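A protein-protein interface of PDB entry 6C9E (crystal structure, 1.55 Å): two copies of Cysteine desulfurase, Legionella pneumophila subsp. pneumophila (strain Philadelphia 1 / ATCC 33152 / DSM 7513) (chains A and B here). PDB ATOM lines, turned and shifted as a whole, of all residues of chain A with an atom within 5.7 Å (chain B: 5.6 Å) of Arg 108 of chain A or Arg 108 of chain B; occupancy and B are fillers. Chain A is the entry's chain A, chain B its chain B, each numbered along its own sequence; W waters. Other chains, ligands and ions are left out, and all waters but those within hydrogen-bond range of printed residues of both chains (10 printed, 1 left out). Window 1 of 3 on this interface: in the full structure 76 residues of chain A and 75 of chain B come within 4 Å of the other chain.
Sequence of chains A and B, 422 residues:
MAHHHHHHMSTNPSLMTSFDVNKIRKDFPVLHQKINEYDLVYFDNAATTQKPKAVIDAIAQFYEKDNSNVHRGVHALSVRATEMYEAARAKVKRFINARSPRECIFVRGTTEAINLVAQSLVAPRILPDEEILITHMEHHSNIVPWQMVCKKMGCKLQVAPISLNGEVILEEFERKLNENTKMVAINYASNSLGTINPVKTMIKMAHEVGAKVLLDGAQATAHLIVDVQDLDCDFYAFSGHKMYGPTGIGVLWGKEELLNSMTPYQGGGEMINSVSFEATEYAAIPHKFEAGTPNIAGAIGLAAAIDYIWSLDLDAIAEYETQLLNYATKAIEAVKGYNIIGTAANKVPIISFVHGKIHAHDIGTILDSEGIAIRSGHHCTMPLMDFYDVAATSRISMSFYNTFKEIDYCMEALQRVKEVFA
Arg 108 of chain A touches Gln 266 of chain B, and with the chains exchanged Gln 266 of chain A touches Arg 108 of chain B.
Glu 112 of chain A touches its own counterpart, Glu 112 of chain B.
Glu 112 of chain A touches Gln 266 of chain B, and with the chains exchanged Gln 266 of chain A touches Glu 112 of chain B.
Thr 247 of chain A touches Asn 295 of chain B, and with the chains exchanged Asn 295 of chain A touches Thr 247 of chain B.
Of the 15 pairs that touch across the chains among the printed residues, 13 have their exchanged pair printed and touching as well.
OE2 of Glu 112 of chain A is in salt-bridge range of NH2 of Arg 108 of chain B (2.8 Å).
The side-chain amide nitrogen (NE2) of Gln 266 of chain A is in hydrogen-bond range of the side-chain carboxylate (OE2) of Glu 112 of chain B (3.3 Å).
OE1 of Gln 266 of chain A lies within hydrogen-bond range of NH2 of Arg 108 of chain B (3.0 Å).
OP3 of LLP 242 of chain A sits at hydrogen-bond distance from the side-chain hydroxyl (OG1) of Thr 293 of chain B, 2.7 Å away.
The guanidinium group (NH2) of Arg 108 of chain A lies within hydrogen-bond range of the side-chain amide oxygen (OE1) of Gln 266 of chain B (3.0 Å).
The guanidinium group of Arg 108 of chain A is in salt-bridge range of the side-chain carboxylate of Glu 112 of chain B, 2.8 Å away.
The side-chain hydroxyl of Thr 247 of chain B is in hydrogen-bond range of the side-chain amide oxygen of Asn 295 of chain A, at 2.8 Å.
The side-chain carboxylate (OE2) of Glu 112 of chain A sits at hydrogen-bond distance from the side-chain amide nitrogen (NE2) of Gln 266 of chain B (3.2 Å).
The side-chain hydroxyl of Thr 247 of chain A sits at hydrogen-bond distance from the side-chain amide oxygen of Asn 295 of chain B, 2.8 Å away.
OP1 of LLP 242 of chain A is in hydrogen-bond range of the side-chain hydroxyl of Ser 239 of chain A (2.6 Å).
O of Arg 108 of chain A sits at hydrogen-bond distance from N of Gly 250 of chain A (3.5 Å).
O of Arg 108 of chain B is in hydrogen-bond range of N of Gly 250 of chain B (3.5 Å).
The side-chain amide nitrogen of Asn 295 of chain A is in hydrogen-bond range of the backbone carbonyl oxygen of Gly 248 of chain A (2.9 Å).
The backbone carbonyl oxygen (O) of Gly 248 of chain B is in hydrogen-bond range of the side-chain amide nitrogen (ND2) of Asn 295 of chain B, 2.9 Å away.
O of Arg 108 of chain B is in hydrogen-bond range of N of Ile 249 of chain B (3.0 Å).
Among the printed residues, Asp or Glu carboxylates within 4 Å of a Lys or Arg side-chain nitrogen of the other chain: Arg 108 of chain A with Glu 112 of chain B and Glu 112 of chain A with Arg 108 of chain B.
Phe 106 of chain A touches none of the printed residues of chain B.
Of the printed residues of chain B, Arg 108 of chain A touches Arg 108 (3.5 Å), Glu 112 (2.8 Å) and Gln 266 (3.0 Å).
Of the printed residues of chain B, Glu 112 of chain A touches Arg 108 (2.8 Å), Glu 112 (3.8 Å) and Gln 266 (3.2 Å).
Of the printed residues of chain B, LLP 242 of chain A touches Thr 293.
Ile 249 of chain A touches none of the printed residues of chain B.
Printed residues of chain A within 4 Å of Arg 108 of chain B: Val 107, Arg 108, Glu 112 and Gln 266.
Of the printed residues of chain A, Thr 247 of chain B touches Asn 295 (2.8 Å).
The nearest printed residue of chain A that does not touch Arg 108 of chain B is Thr 293 of chain A (4.1 Å).
Water W6 lies within hydrogen-bond range of the side-chain amide oxygen of Gln 266 of chain B (2.6 Å), the backbone carbonyl oxygen of Ala 291 of chain B (2.7 Å) and the guanidinium group of Arg 108 of chain A (3.2 Å).
Water W3 lies within hydrogen-bond range of OP2 of LLP 242 of chain A and the backbone carbonyl oxygen (O) of Thr 293 of chain B.
Water W7 lies within hydrogen-bond range of O of Gly 248 of chain A (2.8 Å) and O of Gly 248 of chain B (2.8 Å).
Water W4 lies within hydrogen-bond range of the backbone NH of Ala 291 of chain B, the guanidinium group of Arg 108 of chain A and the side-chain amide oxygen of Gln 266 of chain B.
Water W1 lies within hydrogen-bond range of the backbone NH (N) of Ala 291 of chain A (3.0 Å), the side-chain amide oxygen (OE1) of Gln 266 of chain A (3.2 Å) and the guanidinium group (NH2) of Arg 108 of chain B (3.4 Å).
Water W9 lies within hydrogen-bond range of the backbone carbonyl oxygen of Val 107 of chain A (3.0 Å), the guanidinium group of Arg 108 of chain B (3.0 Å), the backbone carbonyl oxygen of Gly 248 of chain A (3.3 Å) and the backbone NH of Arg 108 of chain A (3.5 Å).
Among the printed residues, merely in contact across the chains: Val 107 of chain A with Arg 108 of chain B (3.99 Å), Arg 108 of chain A with Arg 108 of chain B (3.5 Å), Glu 112 of chain A with Glu 112 of chain B (3.8 Å), Gly 248 of chain A with Asn 295 of chain B (3.6 Å), Gln 266 of chain A with Gln 266 of chain B (3.5 Å) and Asn 295 of chain A with Gly 248 of chain B (3.6 Å).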
ATOM      1  N   PHE A 106      21.398  14.675  -4.560  1.00  0.00           N
ATOM      2  CA  PHE A 106      22.395  15.504  -5.246  1.00  0.00           C
ATOM      3  C   PHE A 106      22.159  15.461  -6.751  1.00  0.00           C
ATOM      4  O   PHE A 106      22.010  14.381  -7.345  1.00  0.00           O
ATOM      5  CB  PHE A 106      23.822  15.027  -4.938  1.00  0.00           C
ATOM      6  CG  PHE A 106      24.296  15.391  -3.562  1.00  0.00           C
ATOM      7  CD1 PHE A 106      24.630  14.390  -2.640  1.00  0.00           C
ATOM      8  CD2 PHE A 106      24.347  16.724  -3.159  1.00  0.00           C
ATOM      9  CE1 PHE A 106      25.075  14.734  -1.344  1.00  0.00           C
ATOM     10  CE2 PHE A 106      24.778  17.078  -1.863  1.00  0.00           C
ATOM     11  CZ  PHE A 106      25.144  16.061  -0.947  1.00  0.00           C
ATOM     12  N   VAL A 107      22.126  16.655  -7.359  1.00  0.00           N
ATOM     13  CA  VAL A 107      21.949  16.865  -8.794  1.00  0.00           C
ATOM     14  C   VAL A 107      23.011  17.862  -9.248  1.00  0.00           C
ATOM     15  O   VAL A 107      23.912  18.218  -8.479  1.00  0.00           O
ATOM     16  CB  VAL A 107      20.522  17.355  -9.105  1.00  0.00           C
ATOM     17  CG1 VAL A 107      19.487  16.247  -8.826  1.00  0.00           C
ATOM     18  CG2 VAL A 107      20.177  18.626  -8.271  1.00  0.00           C
ATOM     19  N   ARG A 108      22.934  18.319 -10.511  1.00  0.00           N
ATOM     20  CA  ARG A 108      23.894  19.319 -10.983  1.00  0.00           C
ATOM     21  C   ARG A 108      23.562  20.719 -10.467  1.00  0.00           C
ATOM     22  O   ARG A 108      24.475  21.533 -10.251  1.00  0.00           O
ATOM     23  CB  ARG A 108      23.948  19.314 -12.512  1.00  0.00           C
ATOM     24  CG  ARG A 108      24.748  20.502 -13.114  1.00  0.00           C
ATOM     25  CD  ARG A 108      25.032  20.307 -14.632  1.00  0.00           C
ATOM     26  NE  ARG A 108      23.845  19.798 -15.297  1.00  0.00           N
ATOM     27  CZ  ARG A 108      23.725  18.538 -15.711  1.00  0.00           C
ATOM     28  NH1 ARG A 108      24.751  17.695 -15.575  1.00  0.00           N
ATOM     29  NH2 ARG A 108      22.602  18.119 -16.263  1.00  0.00           N
ATOM     30  N   GLY A 109      22.288  20.993 -10.220  1.00  0.00           N
ATOM     31  CA  GLY A 109      21.872  22.340  -9.899  1.00  0.00           C
ATOM     32  C   GLY A 109      20.364  22.409  -9.841  1.00  0.00           C
ATOM     33  O   GLY A 109      19.663  21.415 -10.065  1.00  0.00           O
ATOM     34  N   THR A 110      19.885  23.622  -9.530  1.00  0.00           N
ATOM     35  CA  THR A 110      18.450  23.883  -9.451  1.00  0.00           C
ATOM     36  C   THR A 110      17.746  23.457 -10.727  1.00  0.00           C
ATOM     37  O   THR A 110      16.668  22.855 -10.679  1.00  0.00           O
ATOM     38  CB  THR A 110      18.205  25.377  -9.227  1.00  0.00           C
ATOM     39  OG1 THR A 110      18.859  25.806  -8.029  1.00  0.00           O
ATOM     40  CG2 THR A 110      16.710  25.688  -9.129  1.00  0.00           C
ATOM     41  N   GLU A 112      18.470  21.085 -12.948  1.00  0.00           N
ATOM     42  CA  GLU A 112      18.250  19.642 -13.037  1.00  0.00           C
ATOM     43  C   GLU A 112      17.195  19.187 -12.031  1.00  0.00           C
ATOM     44  O   GLU A 112      16.365  18.311 -12.342  1.00  0.00           O
ATOM     45  CB  GLU A 112      19.544  18.874 -12.816  1.00  0.00           C
ATOM     46  CG  GLU A 112      19.294  17.361 -12.917  1.00  0.00           C
ATOM     47  CD  GLU A 112      20.559  16.549 -13.031  1.00  0.00           C
ATOM     48  OE1 GLU A 112      21.573  16.923 -12.415  1.00  0.00           O
ATOM     49  OE2 GLU A 112      20.531  15.506 -13.718  1.00  0.00           O
ATOM     50  N   SER A 239      21.118  25.471  -5.801  1.00  0.00           N
ATOM     51  CA  SER A 239      22.384  25.291  -6.518  1.00  0.00           C
ATOM     52  C   SER A 239      23.559  25.650  -5.627  1.00  0.00           C
ATOM     53  O   SER A 239      23.587  26.740  -5.036  1.00  0.00           O
ATOM     54  CB  SER A 239      22.482  26.179  -7.762  1.00  0.00           C
ATOM     55  OG  SER A 239      21.513  25.860  -8.746  1.00  0.00           O
ATOM     56  N   GLY A 240      24.575  24.787  -5.625  1.00  0.00           N
ATOM     57  CA  GLY A 240      25.738  25.059  -4.794  1.00  0.00           C
ATOM     58  C   GLY A 240      26.467  26.341  -5.168  1.00  0.00           C
ATOM     59  O   GLY A 240      26.964  27.055  -4.287  1.00  0.00           O
ATOM     60  N1  LLP A 242      16.098  29.852 -10.353  1.00  0.00           N
ATOM     61  C2  LLP A 242      16.658  30.988  -9.920  1.00  0.00           C
ATOM     62  C2' LLP A 242      15.788  31.953  -9.169  1.00  0.00           C
ATOM     63  C3  LLP A 242      18.018  31.258 -10.139  1.00  0.00           C
ATOM     64  O3  LLP A 242      18.502  32.441  -9.723  1.00  0.00           O
ATOM     65  C4  LLP A 242      18.810  30.322 -10.819  1.00  0.00           C
ATOM     66  C4' LLP A 242      20.299  30.508 -11.022  1.00  0.00           C
ATOM     67  C5  LLP A 242      18.195  29.159 -11.294  1.00  0.00           C
ATOM     68  C6  LLP A 242      16.859  28.985 -11.028  1.00  0.00           C
ATOM     69  C5' LLP A 242      18.942  28.140 -12.110  1.00  0.00           C
ATOM     70  OP4 LLP A 242      20.062  27.602 -11.318  1.00  0.00           O
ATOM     71  P   LLP A 242      21.305  26.870 -12.073  1.00  0.00           P
ATOM     72  OP1 LLP A 242      22.353  26.679 -11.021  1.00  0.00           O
ATOM     73  OP2 LLP A 242      20.750  25.533 -12.565  1.00  0.00           O
ATOM     74  OP3 LLP A 242      21.728  27.778 -13.192  1.00  0.00           O
ATOM     75  N   LLP A 242      25.594  29.124  -6.223  1.00  0.00           N
ATOM     76  CA  LLP A 242      24.942  30.385  -5.820  1.00  0.00           C
ATOM     77  CB  LLP A 242      23.469  30.403  -6.253  1.00  0.00           C
ATOM     78  CG  LLP A 242      23.561  30.727  -7.733  1.00  0.00           C
ATOM     79  CD  LLP A 242      22.246  30.555  -8.427  1.00  0.00           C
ATOM     80  CE  LLP A 242      22.217  31.213  -9.772  1.00  0.00           C
ATOM     81  NZ  LLP A 242      20.836  31.504 -10.132  1.00  0.00           N
ATOM     82  C   LLP A 242      25.005  30.606  -4.304  1.00  0.00           C
ATOM     83  O   LLP A 242      24.519  31.595  -3.822  1.00  0.00           O
ATOM     84  N   THR A 247      30.851  24.720  -8.562  1.00  0.00           N
ATOM     85  CA  THR A 247      29.946  24.495  -9.681  1.00  0.00           C
ATOM     86  C   THR A 247      29.630  23.004  -9.797  1.00  0.00           C
ATOM     87  O   THR A 247      30.324  22.138  -9.233  1.00  0.00           O
ATOM     88  CB  THR A 247      30.558  24.994 -10.995  1.00  0.00           C
ATOM     89  OG1 THR A 247      31.806  24.316 -11.260  1.00  0.00           O
ATOM     90  CG2 THR A 247      30.838  26.495 -10.930  1.00  0.00           C
ATOM     91  N   GLY A 248      28.565  22.706 -10.538  1.00  0.00           N
ATOM     92  CA  GLY A 248      28.268  21.324 -10.852  1.00  0.00           C
ATOM     93  C   GLY A 248      27.571  20.540  -9.765  1.00  0.00           C
ATOM     94  O   GLY A 248      27.470  19.306  -9.891  1.00  0.00           O
ATOM     95  N   ILE A 249      27.087  21.191  -8.706  1.00  0.00           N
ATOM     96  CA  ILE A 249      26.410  20.490  -7.619  1.00  0.00           C
ATOM     97  C   ILE A 249      25.183  21.289  -7.174  1.00  0.00           C
ATOM     98  O   ILE A 249      25.226  22.520  -7.016  1.00  0.00           O
ATOM     99  CB  ILE A 249      27.376  20.204  -6.437  1.00  0.00           C
ATOM    100  CG1 ILE A 249      26.739  19.239  -5.433  1.00  0.00           C
ATOM    101  CG2 ILE A 249      27.828  21.513  -5.719  1.00  0.00           C
ATOM    102  CD1 ILE A 249      26.641  17.797  -5.940  1.00  0.00           C
ATOM    103  N   GLY A 250      24.093  20.578  -6.945  1.00  0.00           N
ATOM    104  CA  GLY A 250      22.911  21.209  -6.392  1.00  0.00           C
ATOM    105  C   GLY A 250      22.124  20.133  -5.680  1.00  0.00           C
ATOM    106  O   GLY A 250      22.554  18.977  -5.581  1.00  0.00           O
ATOM    107  N   GLN A 266      16.967   9.494 -14.148  1.00  0.00           N
ATOM    108  CA  GLN A 266      18.002   8.853 -14.953  1.00  0.00           C
ATOM    109  C   GLN A 266      18.232   7.425 -14.472  1.00  0.00           C
ATOM    110  O   GLN A 266      18.150   7.140 -13.277  1.00  0.00           O
ATOM    111  CB  GLN A 266      19.304   9.658 -14.896  1.00  0.00           C
ATOM    112  CG  GLN A 266      19.076  11.033 -15.559  1.00  0.00           C
ATOM    113  CD  GLN A 266      20.253  11.965 -15.447  1.00  0.00           C
ATOM    114  OE1 GLN A 266      21.248  11.659 -14.806  1.00  0.00           O
ATOM    115  NE2 GLN A 266      20.137  13.130 -16.069  1.00  0.00           N
ATOM    116  N   ALA A 291      21.988   8.367 -10.493  1.00  0.00           N
ATOM    117  CA  ALA A 291      22.418   7.378 -11.481  1.00  0.00           C
ATOM    118  C   ALA A 291      23.859   7.621 -11.909  1.00  0.00           C
ATOM    119  O   ALA A 291      24.218   8.746 -12.277  1.00  0.00           O
ATOM    120  CB  ALA A 291      21.506   7.448 -12.706  1.00  0.00           C
ATOM    121  N   THR A 293      28.174   7.486 -11.221  1.00  0.00           N
ATOM    122  CA  THR A 293      29.036   8.120 -10.228  1.00  0.00           C
ATOM    123  C   THR A 293      28.561   9.544  -9.944  1.00  0.00           C
ATOM    124  O   THR A 293      28.404  10.349 -10.881  1.00  0.00           O
ATOM    125  CB  THR A 293      30.484   8.134 -10.737  1.00  0.00           C
ATOM    126  OG1 THR A 293      30.894   6.795 -11.059  1.00  0.00           O
ATOM    127  CG2 THR A 293      31.428   8.708  -9.666  1.00  0.00           C
ATOM    128  N   PRO A 294      28.324   9.897  -8.694  1.00  0.00           N
ATOM    129  CA  PRO A 294      27.875  11.251  -8.380  1.00  0.00           C
ATOM    130  C   PRO A 294      29.035  12.225  -8.430  1.00  0.00           C
ATOM    131  O   PRO A 294      30.194  11.843  -8.545  1.00  0.00           O
ATOM    132  CB  PRO A 294      27.322  11.134  -6.959  1.00  0.00           C
ATOM    133  CG  PRO A 294      27.953   9.967  -6.383  1.00  0.00           C
ATOM    134  CD  PRO A 294      28.413   9.033  -7.507  1.00  0.00           C
ATOM    135  N   ASN A 295      28.698  13.515  -8.332  1.00  0.00           N
ATOM    136  CA  ASN A 295      29.745  14.525  -8.213  1.00  0.00           C
ATOM    137  C   ASN A 295      30.228  14.536  -6.766  1.00  0.00           C
ATOM    138  O   ASN A 295      29.817  15.352  -5.943  1.00  0.00           O
ATOM    139  CB  ASN A 295      29.245  15.901  -8.639  1.00  0.00           C
ATOM    140  CG  ASN A 295      30.343  16.931  -8.614  1.00  0.00           C
ATOM    141  OD1 ASN A 295      31.492  16.613  -8.302  1.00  0.00           O
ATOM    142  ND2 ASN A 295      30.006  18.184  -8.942  1.00  0.00           N
ATOM    143  N   PHE B 106      28.718  18.963 -22.593  1.00  0.00           N
ATOM    144  CA  PHE B 106      29.107  18.639 -21.221  1.00  0.00           C
ATOM    145  C   PHE B 106      27.908  18.158 -20.415  1.00  0.00           C
ATOM    146  O   PHE B 106      26.848  18.801 -20.388  1.00  0.00           O
ATOM    147  CB  PHE B 106      29.758  19.846 -20.538  1.00  0.00           C
ATOM    148  CG  PHE B 106      31.159  20.142 -21.027  1.00  0.00           C
ATOM    149  CD1 PHE B 106      32.182  19.191 -20.909  1.00  0.00           C
ATOM    150  CD2 PHE B 106      31.459  21.380 -21.596  1.00  0.00           C
ATOM    151  CE1 PHE B 106      33.450  19.476 -21.381  1.00  0.00           C
ATOM    152  CE2 PHE B 106      32.728  21.667 -22.037  1.00  0.00           C
ATOM    153  CZ  PHE B 106      33.726  20.741 -21.918  1.00  0.00           C
ATOM    154  N   VAL B 107      28.110  17.032 -19.719  1.00  0.00           N
ATOM    155  CA  VAL B 107      27.111  16.376 -18.880  1.00  0.00           C
ATOM    156  C   VAL B 107      27.798  16.017 -17.568  1.00  0.00           C
ATOM    157  O   VAL B 107      28.946  16.402 -17.351  1.00  0.00           O
ATOM    158  CB  VAL B 107      26.545  15.124 -19.574  1.00  0.00           C
ATOM    159  CG1 VAL B 107      25.715  15.522 -20.792  1.00  0.00           C
ATOM    160  CG2 VAL B 107      27.670  14.162 -19.977  1.00  0.00           C
ATOM    161  N   ARG B 108      27.103  15.293 -16.672  1.00  0.00           N
ATOM    162  CA  ARG B 108      27.730  14.853 -15.421  1.00  0.00           C
ATOM    163  C   ARG B 108      28.680  13.682 -15.636  1.00  0.00           C
ATOM    164  O   ARG B 108      29.674  13.560 -14.913  1.00  0.00           O
ATOM    165  CB  ARG B 108      26.651  14.468 -14.397  1.00  0.00           C
ATOM    166  CG  ARG B 108      27.217  13.790 -13.106  1.00  0.00           C
ATOM    167  CD  ARG B 108      26.164  13.640 -11.998  1.00  0.00           C
ATOM    168  NE  ARG B 108      24.873  13.301 -12.547  1.00  0.00           N
ATOM    169  CZ  ARG B 108      23.871  14.169 -12.679  1.00  0.00           C
ATOM    170  NH1 ARG B 108      24.020  15.421 -12.245  1.00  0.00           N
ATOM    171  NH2 ARG B 108      22.731  13.790 -13.249  1.00  0.00           N
ATOM    172  N   GLY B 109      28.406  12.834 -16.619  1.00  0.00           N
ATOM    173  CA  GLY B 109      29.134  11.586 -16.751  1.00  0.00           C
ATOM    174  C   GLY B 109      28.554  10.753 -17.866  1.00  0.00           C
ATOM    175  O   GLY B 109      27.564  11.133 -18.509  1.00  0.00           O
ATOM    176  N   THR B 110      29.195   9.601 -18.086  1.00  0.00           N
ATOM    177  CA  THR B 110      28.724   8.659 -19.103  1.00  0.00           C
ATOM    178  C   THR B 110      27.250   8.322 -18.903  1.00  0.00           C
ATOM    179  O   THR B 110      26.482   8.232 -19.876  1.00  0.00           O
ATOM    180  CB  THR B 110      29.557   7.380 -19.049  1.00  0.00           C
ATOM    181  OG1 THR B 110      30.951   7.671 -19.283  1.00  0.00           O
ATOM    182  CG2 THR B 110      29.069   6.369 -20.095  1.00  0.00           C
ATOM    183  N   GLU B 112      24.743  10.043 -17.571  1.00  0.00           N
ATOM    184  CA  GLU B 112      23.820  11.074 -18.045  1.00  0.00           C
ATOM    185  C   GLU B 112      23.837  11.163 -19.565  1.00  0.00           C
ATOM    186  O   GLU B 112      22.782  11.340 -20.193  1.00  0.00           O
ATOM    187  CB  GLU B 112      24.160  12.433 -17.422  1.00  0.00           C
ATOM    188  CG  GLU B 112      23.229  13.507 -17.994  1.00  0.00           C
ATOM    189  CD  GLU B 112      23.284  14.791 -17.234  1.00  0.00           C
ATOM    190  OE1 GLU B 112      24.365  15.174 -16.756  1.00  0.00           O
ATOM    191  OE2 GLU B 112      22.224  15.428 -17.116  1.00  0.00           O
ATOM    192  N   SER B 239      33.373   9.710 -19.150  1.00  0.00           N
ATOM    193  CA  SER B 239      33.360  10.349 -17.837  1.00  0.00           C
ATOM    194  C   SER B 239      34.731  10.894 -17.476  1.00  0.00           C
ATOM    195  O   SER B 239      35.723  10.158 -17.527  1.00  0.00           O
ATOM    196  CB  SER B 239      32.972   9.357 -16.732  1.00  0.00           C
ATOM    197  OG  SER B 239      31.656   8.865 -16.903  1.00  0.00           O
ATOM    198  N   THR B 247      35.472  14.751 -10.605  1.00  0.00           N
ATOM    199  CA  THR B 247      34.125  14.183 -10.592  1.00  0.00           C
ATOM    200  C   THR B 247      33.111  15.200 -11.119  1.00  0.00           C
ATOM    201  O   THR B 247      33.369  16.408 -11.199  1.00  0.00           O
ATOM    202  CB  THR B 247      33.725  13.747  -9.170  1.00  0.00           C
ATOM    203  OG1 THR B 247      33.735  14.869  -8.260  1.00  0.00           O
ATOM    204  CG2 THR B 247      34.706  12.715  -8.658  1.00  0.00           C
ATOM    205  N   GLY B 248      31.947  14.678 -11.492  1.00  0.00           N
ATOM    206  CA  GLY B 248      30.841  15.545 -11.875  1.00  0.00           C
ATOM    207  C   GLY B 248      30.898  16.104 -13.274  1.00  0.00           C
ATOM    208  O   GLY B 248      30.132  17.040 -13.565  1.00  0.00           O
ATOM    209  N   ILE B 249      31.784  15.605 -14.138  1.00  0.00           N
ATOM    210  CA  ILE B 249      31.891  16.108 -15.510  1.00  0.00           C
ATOM    211  C   ILE B 249      32.078  14.927 -16.454  1.00  0.00           C
ATOM    212  O   ILE B 249      32.822  13.984 -16.158  1.00  0.00           O
ATOM    213  CB  ILE B 249      33.028  17.151 -15.654  1.00  0.00           C
ATOM    214  CG1 ILE B 249      32.964  17.881 -16.995  1.00  0.00           C
ATOM    215  CG2 ILE B 249      34.426  16.524 -15.474  1.00  0.00           C
ATOM    216  CD1 ILE B 249      31.739  18.796 -17.138  1.00  0.00           C
ATOM    217  N   GLY B 250      31.401  14.989 -17.590  1.00  0.00           N
ATOM    218  CA  GLY B 250      31.572  14.001 -18.637  1.00  0.00           C
ATOM    219  C   GLY B 250      31.161  14.630 -19.944  1.00  0.00           C
ATOM    220  O   GLY B 250      30.819  15.812 -20.001  1.00  0.00           O
ATOM    221  N   GLN B 266      17.113  18.278 -20.832  1.00  0.00           N
ATOM    222  CA  GLN B 266      16.657  19.149 -19.752  1.00  0.00           C
ATOM    223  C   GLN B 266      16.376  20.549 -20.284  1.00  0.00           C
ATOM    224  O   GLN B 266      17.066  21.046 -21.176  1.00  0.00           O
ATOM    225  CB  GLN B 266      17.708  19.201 -18.632  1.00  0.00           C
ATOM    226  CG  GLN B 266      17.809  17.827 -17.972  1.00  0.00           C
ATOM    227  CD  GLN B 266      18.946  17.697 -16.977  1.00  0.00           C
ATOM    228  OE1 GLN B 266      19.638  18.649 -16.669  1.00  0.00           O
ATOM    229  NE2 GLN B 266      19.113  16.490 -16.440  1.00  0.00           N
ATOM    230  N   ALA B 291      21.452  22.766 -19.916  1.00  0.00           N
ATOM    231  CA  ALA B 291      20.395  23.509 -19.241  1.00  0.00           C
ATOM    232  C   ALA B 291      20.882  23.979 -17.884  1.00  0.00           C
ATOM    233  O   ALA B 291      21.353  23.171 -17.081  1.00  0.00           O
ATOM    234  CB  ALA B 291      19.147  22.635 -19.068  1.00  0.00           C
ATOM    235  N   THR B 293      23.244  26.593 -15.280  1.00  0.00           N
ATOM    236  CA  THR B 293      24.679  26.818 -15.120  1.00  0.00           C
ATOM    237  C   THR B 293      25.439  25.505 -15.264  1.00  0.00           C
ATOM    238  O   THR B 293      25.131  24.531 -14.567  1.00  0.00           O
ATOM    239  CB  THR B 293      24.980  27.430 -13.747  1.00  0.00           C
ATOM    240  OG1 THR B 293      24.254  28.648 -13.568  1.00  0.00           O
ATOM    241  CG2 THR B 293      26.504  27.696 -13.588  1.00  0.00           C
ATOM    242  N   PRO B 294      26.427  25.436 -16.134  1.00  0.00           N
ATOM    243  CA  PRO B 294      27.144  24.179 -16.324  1.00  0.00           C
ATOM    244  C   PRO B 294      28.157  23.982 -15.209  1.00  0.00           C
ATOM    245  O   PRO B 294      28.397  24.866 -14.390  1.00  0.00           O
ATOM    246  CB  PRO B 294      27.822  24.343 -17.690  1.00  0.00           C
ATOM    247  CG  PRO B 294      27.846  25.803 -17.947  1.00  0.00           C
ATOM    248  CD  PRO B 294      26.846  26.493 -17.069  1.00  0.00           C
ATOM    249  N   ASN B 295      28.733  22.785 -15.173  1.00  0.00           N
ATOM    250  CA  ASN B 295      29.845  22.542 -14.262  1.00  0.00           C
ATOM    251  C   ASN B 295      31.104  23.163 -14.866  1.00  0.00           C
ATOM    252  O   ASN B 295      31.938  22.488 -15.473  1.00  0.00           O
ATOM    253  CB  ASN B 295      30.025  21.055 -14.012  1.00  0.00           C
ATOM    254  CG  ASN B 295      31.087  20.806 -13.002  1.00  0.00           C
ATOM    255  OD1 ASN B 295      31.672  21.747 -12.471  1.00  0.00           O
ATOM    256  ND2 ASN B 295      31.309  19.532 -12.667  1.00  0.00           N
HETATM  257  O   HOH W   1      21.569  11.061 -11.643  1.00  0.00           O
HETATM  258  O   HOH W   2      27.777  18.455 -15.317  1.00  0.00           O
HETATM  259  O   HOH W   3      22.866  23.967 -12.987  1.00  0.00           O
HETATM  260  O   HOH W   4      21.895  20.124 -18.765  1.00  0.00           O
HETATM  261  O   HOH W   5      31.378  12.028 -11.226  1.00  0.00           O
HETATM  262  O   HOH W   6      20.839  20.782 -15.834  1.00  0.00           O
HETATM  263  O   HOH W   7      27.813  17.611 -12.078  1.00  0.00           O
HETATM  264  O   HOH W   8      23.644  10.747 -14.099  1.00  0.00           O
HETATM  265  O   HOH W   9      25.829  16.468 -10.025  1.00  0.00           O
HETATM  266  O   HOH W  10      27.088  24.624 -11.789  1.00  0.00           O
